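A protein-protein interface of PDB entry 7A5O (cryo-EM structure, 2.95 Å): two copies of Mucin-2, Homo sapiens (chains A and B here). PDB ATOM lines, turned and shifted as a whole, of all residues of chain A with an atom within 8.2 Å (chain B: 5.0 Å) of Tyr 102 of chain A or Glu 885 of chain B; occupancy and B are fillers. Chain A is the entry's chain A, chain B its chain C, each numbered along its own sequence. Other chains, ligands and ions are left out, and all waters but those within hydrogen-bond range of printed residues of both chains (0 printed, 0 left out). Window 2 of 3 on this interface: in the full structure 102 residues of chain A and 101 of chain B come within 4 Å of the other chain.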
ATOM      1  N   LEU A  92      18.280  37.983  -5.116  1.00  0.00           N
ATOM      2  CA  LEU A  92      17.378  37.412  -4.124  1.00  0.00           C
ATOM      3  C   LEU A  92      17.722  38.000  -2.768  1.00  0.00           C
ATOM      4  O   LEU A  92      18.801  37.723  -2.235  1.00  0.00           O
ATOM      5  CB  LEU A  92      17.491  35.893  -4.092  1.00  0.00           C
ATOM      6  CG  LEU A  92      16.715  35.113  -3.030  1.00  0.00           C
ATOM      7  CD1 LEU A  92      15.233  35.274  -3.150  1.00  0.00           C
ATOM      8  CD2 LEU A  92      17.078  33.661  -3.120  1.00  0.00           C
ATOM      9  N   VAL A  97      22.624  36.244  -6.865  1.00  0.00           N
ATOM     10  CA  VAL A  97      22.649  34.786  -6.888  1.00  0.00           C
ATOM     11  C   VAL A  97      23.387  34.307  -8.129  1.00  0.00           C
ATOM     12  O   VAL A  97      23.317  34.926  -9.197  1.00  0.00           O
ATOM     13  CB  VAL A  97      21.239  34.163  -6.804  1.00  0.00           C
ATOM     14  CG1 VAL A  97      20.604  34.504  -5.491  1.00  0.00           C
ATOM     15  CG2 VAL A  97      20.358  34.609  -7.924  1.00  0.00           C
ATOM     16  N   SER A  98      24.145  33.231  -7.959  1.00  0.00           N
ATOM     17  CA  SER A  98      24.702  32.476  -9.066  1.00  0.00           C
ATOM     18  C   SER A  98      23.670  31.458  -9.514  1.00  0.00           C
ATOM     19  O   SER A  98      23.128  30.717  -8.692  1.00  0.00           O
ATOM     20  CB  SER A  98      25.985  31.765  -8.648  1.00  0.00           C
ATOM     21  OG  SER A  98      25.705  30.786  -7.668  1.00  0.00           O
ATOM     22  N   THR A  99      23.403  31.425 -10.807  1.00  0.00           N
ATOM     23  CA  THR A  99      22.339  30.537 -11.244  1.00  0.00           C
ATOM     24  C   THR A  99      22.913  29.252 -11.824  1.00  0.00           C
ATOM     25  O   THR A  99      23.945  29.288 -12.496  1.00  0.00           O
ATOM     26  CB  THR A  99      21.471  31.226 -12.292  1.00  0.00           C
ATOM     27  OG1 THR A  99      22.286  31.588 -13.409  1.00  0.00           O
ATOM     28  CG2 THR A  99      20.828  32.463 -11.708  1.00  0.00           C
ATOM     29  N   PRO A 100      22.284  28.082 -11.615  1.00  0.00           N
ATOM     30  CA  PRO A 100      21.006  27.781 -10.956  1.00  0.00           C
ATOM     31  C   PRO A 100      21.036  27.839  -9.436  1.00  0.00           C
ATOM     32  O   PRO A 100      22.075  27.645  -8.827  1.00  0.00           O
ATOM     33  CB  PRO A 100      20.711  26.363 -11.422  1.00  0.00           C
ATOM     34  CG  PRO A 100      22.022  25.795 -11.683  1.00  0.00           C
ATOM     35  CD  PRO A 100      22.880  26.878 -12.203  1.00  0.00           C
ATOM     36  N   HIS A 101      19.879  28.100  -8.840  1.00  0.00           N
ATOM     37  CA  HIS A 101      19.740  28.304  -7.405  1.00  0.00           C
ATOM     38  C   HIS A 101      18.634  27.400  -6.890  1.00  0.00           C
ATOM     39  O   HIS A 101      17.503  27.480  -7.368  1.00  0.00           O
ATOM     40  CB  HIS A 101      19.430  29.768  -7.110  1.00  0.00           C
ATOM     41  CG  HIS A 101      19.294  30.079  -5.658  1.00  0.00           C
ATOM     42  ND1 HIS A 101      20.371  30.123  -4.804  1.00  0.00           N
ATOM     43  CD2 HIS A 101      18.208  30.384  -4.912  1.00  0.00           C
ATOM     44  CE1 HIS A 101      19.953  30.427  -3.589  1.00  0.00           C
ATOM     45  NE2 HIS A 101      18.644  30.591  -3.628  1.00  0.00           N
ATOM     46  N   TYR A 102      18.949  26.562  -5.899  1.00  0.00           N
ATOM     47  CA  TYR A 102      18.182  25.349  -5.633  1.00  0.00           C
ATOM     48  C   TYR A 102      17.520  25.307  -4.258  1.00  0.00           C
ATOM     49  O   TYR A 102      17.330  24.207  -3.730  1.00  0.00           O
ATOM     50  CB  TYR A 102      19.080  24.117  -5.754  1.00  0.00           C
ATOM     51  CG  TYR A 102      19.630  23.781  -7.124  1.00  0.00           C
ATOM     52  CD1 TYR A 102      18.847  23.135  -8.066  1.00  0.00           C
ATOM     53  CD2 TYR A 102      20.955  24.045  -7.440  1.00  0.00           C
ATOM     54  CE1 TYR A 102      19.349  22.805  -9.302  1.00  0.00           C
ATOM     55  CE2 TYR A 102      21.469  23.716  -8.670  1.00  0.00           C
ATOM     56  CZ  TYR A 102      20.662  23.096  -9.599  1.00  0.00           C
ATOM     57  OH  TYR A 102      21.162  22.757 -10.833  1.00  0.00           O
ATOM     58  N   SER A 103      17.183  26.451  -3.656  1.00  0.00           N
ATOM     59  CA  SER A 103      16.613  26.455  -2.308  1.00  0.00           C
ATOM     60  C   SER A 103      15.230  25.796  -2.305  1.00  0.00           C
ATOM     61  O   SER A 103      14.489  25.902  -3.283  1.00  0.00           O
ATOM     62  CB  SER A 103      16.524  27.882  -1.769  1.00  0.00           C
ATOM     63  OG  SER A 103      15.573  28.645  -2.479  1.00  0.00           O
ATOM     64  N   PRO A 104      14.846  25.098  -1.203  1.00  0.00           N
ATOM     65  CA  PRO A 104      13.778  24.085  -1.307  1.00  0.00           C
ATOM     66  C   PRO A 104      12.349  24.592  -1.471  1.00  0.00           C
ATOM     67  O   PRO A 104      11.403  23.856  -1.182  1.00  0.00           O
ATOM     68  CB  PRO A 104      13.914  23.304   0.008  1.00  0.00           C
ATOM     69  CG  PRO A 104      15.299  23.531   0.449  1.00  0.00           C
ATOM     70  CD  PRO A 104      15.600  24.937   0.055  1.00  0.00           C
ATOM     71  N   GLY A 105      12.159  25.838  -1.874  1.00  0.00           N
ATOM     72  CA  GLY A 105      10.850  26.259  -2.320  1.00  0.00           C
ATOM     73  C   GLY A 105      10.924  27.096  -3.578  1.00  0.00           C
ATOM     74  O   GLY A 105       9.920  27.667  -4.007  1.00  0.00           O
ATOM     75  N   LEU A 106      12.108  27.165  -4.187  1.00  0.00           N
ATOM     76  CA  LEU A 106      12.372  28.208  -5.172  1.00  0.00           C
ATOM     77  C   LEU A 106      13.547  27.802  -6.045  1.00  0.00           C
ATOM     78  O   LEU A 106      14.660  27.644  -5.544  1.00  0.00           O
ATOM     79  CB  LEU A 106      12.663  29.513  -4.456  1.00  0.00           C
ATOM     80  CG  LEU A 106      12.827  30.801  -5.236  1.00  0.00           C
ATOM     81  CD1 LEU A 106      11.523  31.171  -5.898  1.00  0.00           C
ATOM     82  CD2 LEU A 106      13.277  31.862  -4.276  1.00  0.00           C
ATOM     83  N   LEU A 107      13.310  27.664  -7.343  1.00  0.00           N
ATOM     84  CA  LEU A 107      14.352  27.366  -8.315  1.00  0.00           C
ATOM     85  C   LEU A 107      14.491  28.546  -9.263  1.00  0.00           C
ATOM     86  O   LEU A 107      13.508  28.968  -9.874  1.00  0.00           O
ATOM     87  CB  LEU A 107      14.031  26.088  -9.084  1.00  0.00           C
ATOM     88  CG  LEU A 107      15.014  25.620 -10.154  1.00  0.00           C
ATOM     89  CD1 LEU A 107      16.358  25.324  -9.571  1.00  0.00           C
ATOM     90  CD2 LEU A 107      14.470  24.382 -10.809  1.00  0.00           C
ATOM     91  N   ILE A 108      15.706  29.073  -9.382  1.00  0.00           N
ATOM     92  CA  ILE A 108      16.006  30.231 -10.216  1.00  0.00           C
ATOM     93  C   ILE A 108      17.134  29.822 -11.149  1.00  0.00           C
ATOM     94  O   ILE A 108      18.280  29.684 -10.711  1.00  0.00           O
ATOM     95  CB  ILE A 108      16.423  31.449  -9.380  1.00  0.00           C
ATOM     96  CG1 ILE A 108      15.331  31.855  -8.401  1.00  0.00           C
ATOM     97  CG2 ILE A 108      16.737  32.630 -10.278  1.00  0.00           C
ATOM     98  CD1 ILE A 108      15.802  32.856  -7.406  1.00  0.00           C
ATOM     99  N   GLU A 109      16.834  29.653 -12.430  1.00  0.00           N
ATOM    100  CA  GLU A 109      17.836  29.194 -13.380  1.00  0.00           C
ATOM    101  C   GLU A 109      17.816  30.056 -14.633  1.00  0.00           C
ATOM    102  O   GLU A 109      16.791  30.630 -14.992  1.00  0.00           O
ATOM    103  CB  GLU A 109      17.617  27.724 -13.729  1.00  0.00           C
ATOM    104  CG  GLU A 109      16.310  27.436 -14.414  1.00  0.00           C
ATOM    105  CD  GLU A 109      16.099  25.964 -14.641  1.00  0.00           C
ATOM    106  OE1 GLU A 109      16.976  25.174 -14.242  1.00  0.00           O
ATOM    107  OE2 GLU A 109      15.056  25.591 -15.210  1.00  0.00           O
ATOM    108  N   GLU A 302      14.003  16.738 -16.301  1.00  0.00           N
ATOM    109  CA  GLU A 302      12.693  17.160 -15.798  1.00  0.00           C
ATOM    110  C   GLU A 302      12.281  18.540 -16.312  1.00  0.00           C
ATOM    111  O   GLU A 302      11.816  19.402 -15.566  1.00  0.00           O
ATOM    112  CB  GLU A 302      12.696  17.094 -14.273  1.00  0.00           C
ATOM    113  CG  GLU A 302      13.800  17.894 -13.580  1.00  0.00           C
ATOM    114  CD  GLU A 302      13.781  17.731 -12.074  1.00  0.00           C
ATOM    115  OE1 GLU A 302      12.905  17.010 -11.561  1.00  0.00           O
ATOM    116  OE2 GLU A 302      14.656  18.308 -11.403  1.00  0.00           O
ATOM    117  N   CYS B 862      25.686  23.358  -5.017  1.00  0.00           N
ATOM    118  CA  CYS B 862      25.098  22.977  -6.300  1.00  0.00           C
ATOM    119  C   CYS B 862      24.271  21.723  -6.026  1.00  0.00           C
ATOM    120  O   CYS B 862      24.014  21.383  -4.869  1.00  0.00           O
ATOM    121  CB  CYS B 862      26.175  22.768  -7.373  1.00  0.00           C
ATOM    122  SG  CYS B 862      25.602  22.553  -9.066  1.00  0.00           S
ATOM    123  N   SER B 863      23.839  21.038  -7.079  1.00  0.00           N
ATOM    124  CA  SER B 863      23.329  19.678  -6.971  1.00  0.00           C
ATOM    125  C   SER B 863      24.434  18.694  -7.316  1.00  0.00           C
ATOM    126  O   SER B 863      25.135  18.871  -8.312  1.00  0.00           O
ATOM    127  CB  SER B 863      22.142  19.436  -7.896  1.00  0.00           C
ATOM    128  OG  SER B 863      21.034  20.212  -7.518  1.00  0.00           O
ATOM    129  N   ILE B 883      20.297  12.257  -6.067  1.00  0.00           N
ATOM    130  CA  ILE B 883      20.883  13.587  -6.161  1.00  0.00           C
ATOM    131  C   ILE B 883      20.693  14.263  -4.813  1.00  0.00           C
ATOM    132  O   ILE B 883      19.655  14.089  -4.174  1.00  0.00           O
ATOM    133  CB  ILE B 883      20.197  14.385  -7.289  1.00  0.00           C
ATOM    134  CG1 ILE B 883      20.213  13.603  -8.599  1.00  0.00           C
ATOM    135  CG2 ILE B 883      20.835  15.731  -7.498  1.00  0.00           C
ATOM    136  CD1 ILE B 883      21.552  13.295  -9.112  1.00  0.00           C
ATOM    137  N   THR B 884      21.689  15.017  -4.368  1.00  0.00           N
ATOM    138  CA  THR B 884      21.587  15.817  -3.157  1.00  0.00           C
ATOM    139  C   THR B 884      21.690  17.296  -3.501  1.00  0.00           C
ATOM    140  O   THR B 884      22.405  17.676  -4.427  1.00  0.00           O
ATOM    141  CB  THR B 884      22.657  15.396  -2.133  1.00  0.00           C
ATOM    142  OG1 THR B 884      22.545  16.185  -0.945  1.00  0.00           O
ATOM    143  CG2 THR B 884      24.052  15.468  -2.693  1.00  0.00           C
ATOM    144  N   GLU B 885      20.933  18.131  -2.794  1.00  0.00           N
ATOM    145  CA  GLU B 885      20.906  19.571  -3.051  1.00  0.00           C
ATOM    146  C   GLU B 885      21.441  20.300  -1.832  1.00  0.00           C
ATOM    147  O   GLU B 885      20.744  20.438  -0.830  1.00  0.00           O
ATOM    148  CB  GLU B 885      19.514  20.058  -3.398  1.00  0.00           C
ATOM    149  CG  GLU B 885      19.015  19.511  -4.698  1.00  0.00           C
ATOM    150  CD  GLU B 885      17.660  20.035  -5.056  1.00  0.00           C
ATOM    151  OE1 GLU B 885      17.081  20.771  -4.235  1.00  0.00           O
ATOM    152  OE2 GLU B 885      17.166  19.709  -6.151  1.00  0.00           O
ATOM    153  N   ASN B 886      22.662  20.795  -1.945  1.00  0.00           N
ATOM    154  CA  ASN B 886      23.403  21.361  -0.834  1.00  0.00           C
ATOM    155  C   ASN B 886      23.338  22.880  -0.937  1.00  0.00           C
ATOM    156  O   ASN B 886      23.698  23.447  -1.969  1.00  0.00           O
ATOM    157  CB  ASN B 886      24.845  20.875  -0.894  1.00  0.00           C
ATOM    158  CG  ASN B 886      24.966  19.375  -0.803  1.00  0.00           C
ATOM    159  OD1 ASN B 886      24.309  18.721  -0.007  1.00  0.00           O
ATOM    160  ND2 ASN B 886      25.812  18.819  -1.643  1.00  0.00           N
ATOM    161  N   VAL B 887      22.864  23.533   0.114  1.00  0.00           N
ATOM    162  CA  VAL B 887      22.703  24.986   0.121  1.00  0.00           C
ATOM    163  C   VAL B 887      23.524  25.517   1.287  1.00  0.00           C
ATOM    164  O   VAL B 887      23.862  24.755   2.204  1.00  0.00           O
ATOM    165  CB  VAL B 887      21.216  25.399   0.228  1.00  0.00           C
ATOM    166  CG1 VAL B 887      20.397  24.814  -0.900  1.00  0.00           C
ATOM    167  CG2 VAL B 887      20.654  25.016   1.548  1.00  0.00           C
ATOM    168  N   CYS B 896      25.100  22.439   3.804  1.00  0.00           N
ATOM    169  CA  CYS B 896      24.478  21.218   4.281  1.00  0.00           C
ATOM    170  C   CYS B 896      23.377  20.810   3.317  1.00  0.00           C
ATOM    171  O   CYS B 896      22.922  21.603   2.498  1.00  0.00           O
ATOM    172  CB  CYS B 896      23.953  21.391   5.705  1.00  0.00           C
ATOM    173  SG  CYS B 896      22.774  22.702   5.930  1.00  0.00           S
ATOM    174  N   SER B 897      22.965  19.552   3.416  1.00  0.00           N
ATOM    175  CA  SER B 897      22.039  18.949   2.467  1.00  0.00           C
ATOM    176  C   SER B 897      20.605  19.223   2.877  1.00  0.00           C
ATOM    177  O   SER B 897      20.223  18.955   4.016  1.00  0.00           O
ATOM    178  CB  SER B 897      22.269  17.445   2.379  1.00  0.00           C
ATOM    179  OG  SER B 897      21.369  16.859   1.468  1.00  0.00           O
ATOM    180  N   LYS B 898      19.809  19.754   1.951  1.00  0.00           N
ATOM    181  CA  LYS B 898      18.435  20.109   2.262  1.00  0.00           C
ATOM    182  C   LYS B 898      17.386  19.467   1.369  1.00  0.00           C
ATOM    183  O   LYS B 898      16.197  19.644   1.637  1.00  0.00           O
ATOM    184  CB  LYS B 898      18.249  21.629   2.243  1.00  0.00           C
ATOM    185  CG  LYS B 898      18.997  22.342   3.343  1.00  0.00           C
ATOM    186  CD  LYS B 898      18.530  21.889   4.709  1.00  0.00           C
ATOM    187  CE  LYS B 898      17.126  22.365   5.027  1.00  0.00           C
ATOM    188  NZ  LYS B 898      16.711  21.910   6.381  1.00  0.00           N
ATOM    189  N   ALA B 899      17.773  18.711   0.348  1.00  0.00           N
ATOM    190  CA  ALA B 899      16.801  18.025  -0.490  1.00  0.00           C
ATOM    191  C   ALA B 899      17.450  16.809  -1.126  1.00  0.00           C
ATOM    192  O   ALA B 899      18.649  16.804  -1.396  1.00  0.00           O
ATOM    193  CB  ALA B 899      16.232  18.946  -1.570  1.00  0.00           C
ATOM    194  N   LYS B 901      16.658  13.960  -4.296  1.00  0.00           N
ATOM    195  CA  LYS B 901      15.861  13.533  -5.437  1.00  0.00           C
ATOM    196  C   LYS B 901      16.219  12.100  -5.777  1.00  0.00           C
ATOM    197  O   LYS B 901      17.392  11.789  -5.974  1.00  0.00           O
ATOM    198  CB  LYS B 901      16.083  14.425  -6.658  1.00  0.00           C
ATOM    199  CG  LYS B 901      15.605  15.841  -6.491  1.00  0.00           C
ATOM    200  CD  LYS B 901      15.623  16.584  -7.800  1.00  0.00           C
ATOM    201  CE  LYS B 901      17.033  16.920  -8.235  1.00  0.00           C
ATOM    202  NZ  LYS B 901      17.068  17.766  -9.462  1.00  0.00           N
ATOM    203  N   LYS B 910      10.879  12.953  -4.529  1.00  0.00           N
ATOM    204  CA  LYS B 910      11.677  14.061  -4.030  1.00  0.00           C
ATOM    205  C   LYS B 910      11.381  14.248  -2.557  1.00  0.00           C
ATOM    206  O   LYS B 910      10.215  14.335  -2.172  1.00  0.00           O
ATOM    207  CB  LYS B 910      11.401  15.361  -4.780  1.00  0.00           C
ATOM    208  CG  LYS B 910      12.330  16.463  -4.344  1.00  0.00           C
ATOM    209  CD  LYS B 910      12.195  17.690  -5.180  1.00  0.00           C
ATOM    210  CE  LYS B 910      13.208  18.727  -4.740  1.00  0.00           C
ATOM    211  NZ  LYS B 910      13.113  19.964  -5.559  1.00  0.00           N
ATOM    212  N   ALA B1004      25.266  21.063 -12.526  1.00  0.00           N
ATOM    213  CA  ALA B1004      25.245  22.100 -13.539  1.00  0.00           C
ATOM    214  C   ALA B1004      26.647  22.618 -13.800  1.00  0.00           C
ATOM    215  O   ALA B1004      27.427  22.782 -12.863  1.00  0.00           O
ATOM    216  CB  ALA B1004      24.352  23.258 -13.109  1.00  0.00           C
ATOM    217  N   CYS B1007      27.690  26.024 -11.985  1.00  0.00           N
ATOM    218  CA  CYS B1007      27.950  26.064 -10.560  1.00  0.00           C
ATOM    219  C   CYS B1007      29.438  26.313 -10.319  1.00  0.00           C
ATOM    220  O   CYS B1007      30.280  25.850 -11.089  1.00  0.00           O
ATOM    221  CB  CYS B1007      27.529  24.753  -9.900  1.00  0.00           C
ATOM    222  SG  CYS B1007      25.761  24.407  -9.882  1.00  0.00           S
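The backbone carbonyl oxygen (O) of Tyr 102 of chain A sits close to the side-chain carboxylate (OE1) of Glu 885 of chain B (3.5 Å).
The side-chain amino group (NZ) of Lys 901 of chain B is in salt-bridge range of the side-chain carboxylate (OE2) of Glu 302 of chain A, at 3.1 Å.
The side-chain amino group (NZ) of Lys 901 of chain B lies within salt-bridge range of the side-chain carboxylate (OE2) of Glu 885 of chain B (3.8 Å).
The backbone carbonyl oxygen (O) of Ala 899 of chain B lies within hydrogen-bond range of the backbone NH (N) of Glu 885 of chain B, 3.0 Å away.
The backbone NH (N) of Ala 1004 of chain B is in hydrogen-bond range of the side-chain sulfur (SG) of Cys 862 of chain B (3.8 Å).
The backbone NH (N) of Lys 898 of chain B is in hydrogen-bond range of the backbone carbonyl oxygen (O) of Glu 885 of chain B.
The backbone NH of Ile 883 of chain B lies within hydrogen-bond range of the backbone carbonyl oxygen of Lys 901 of chain B.
The side-chain sulfur of Cys 862 of chain B forms a disulfide with the side-chain sulfur of Cys 1007 of chain B (2.0 Å).
Among the printed residues, pairs that only touch across the chains: Tyr 102 of chain A with Ser 863 of chain B, Pro 100 of chain A with Ala 1004 of chain B, Pro 104 of chain A with Lys 898 of chain B and Tyr 102 of chain A with Ala 1004 of chain B.
Of the printed residues of chain B, Tyr 102 of chain A touches Ser 863 (3.6 Å), Glu 885 (3.5 Å) and Ala 1004 (3.95 Å).
Of chain A, only Tyr 102 (3.5 Å) comes within 4 Å of Glu 885 of chain B.
No residue of chain A comes within 4 Å of Thr 884 of chain B.
Of the printed residues of chain B, Glu 302 of chain A touches Lys 901.
Printed residues of chain A within 4 Å of Ala 1004 of chain B: Pro 100 and Tyr 102.
Printed residues of chain B within 4 Å of Pro 100 of chain A: Ala 1004 (3.7 Å).
Printed residues of chain A within 4 Å of Lys 901 of chain B: Glu 302.
Of the printed residues of chain A, Lys 898 of chain B touches Pro 104 (3.9 Å).
The nearest printed residue of chain A that does not touch Lys 901 of chain B is Tyr 102 of chain A (5.5 Å).
Of the 15 printed residues of chain A, 4 touch a printed residue of chain B.
Printed residues of chain A that touch a printed residue of chain B: Pro 100, Tyr 102, Pro 104 and Glu 302.
Of the 15 printed residues of chain B, 5 touch a printed residue of chain A.
Hydrophobic or aromatic side chains of chain B within 4 Å of the printed part of chain A: Ala 1004.
Among the printed residues, 6 pairs touch across the chains.
Among the printed residues, Asp or Glu carboxylates within 4 Å of a Lys or Arg side-chain nitrogen of the other chain: Glu 302 of chain A with Lys 901 of chain B (3.1 Å).
No position is printed for both chains.
Of the 6 pairs that touch across the chains among the printed residues, none has its exchanged pair printed and touching as well.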
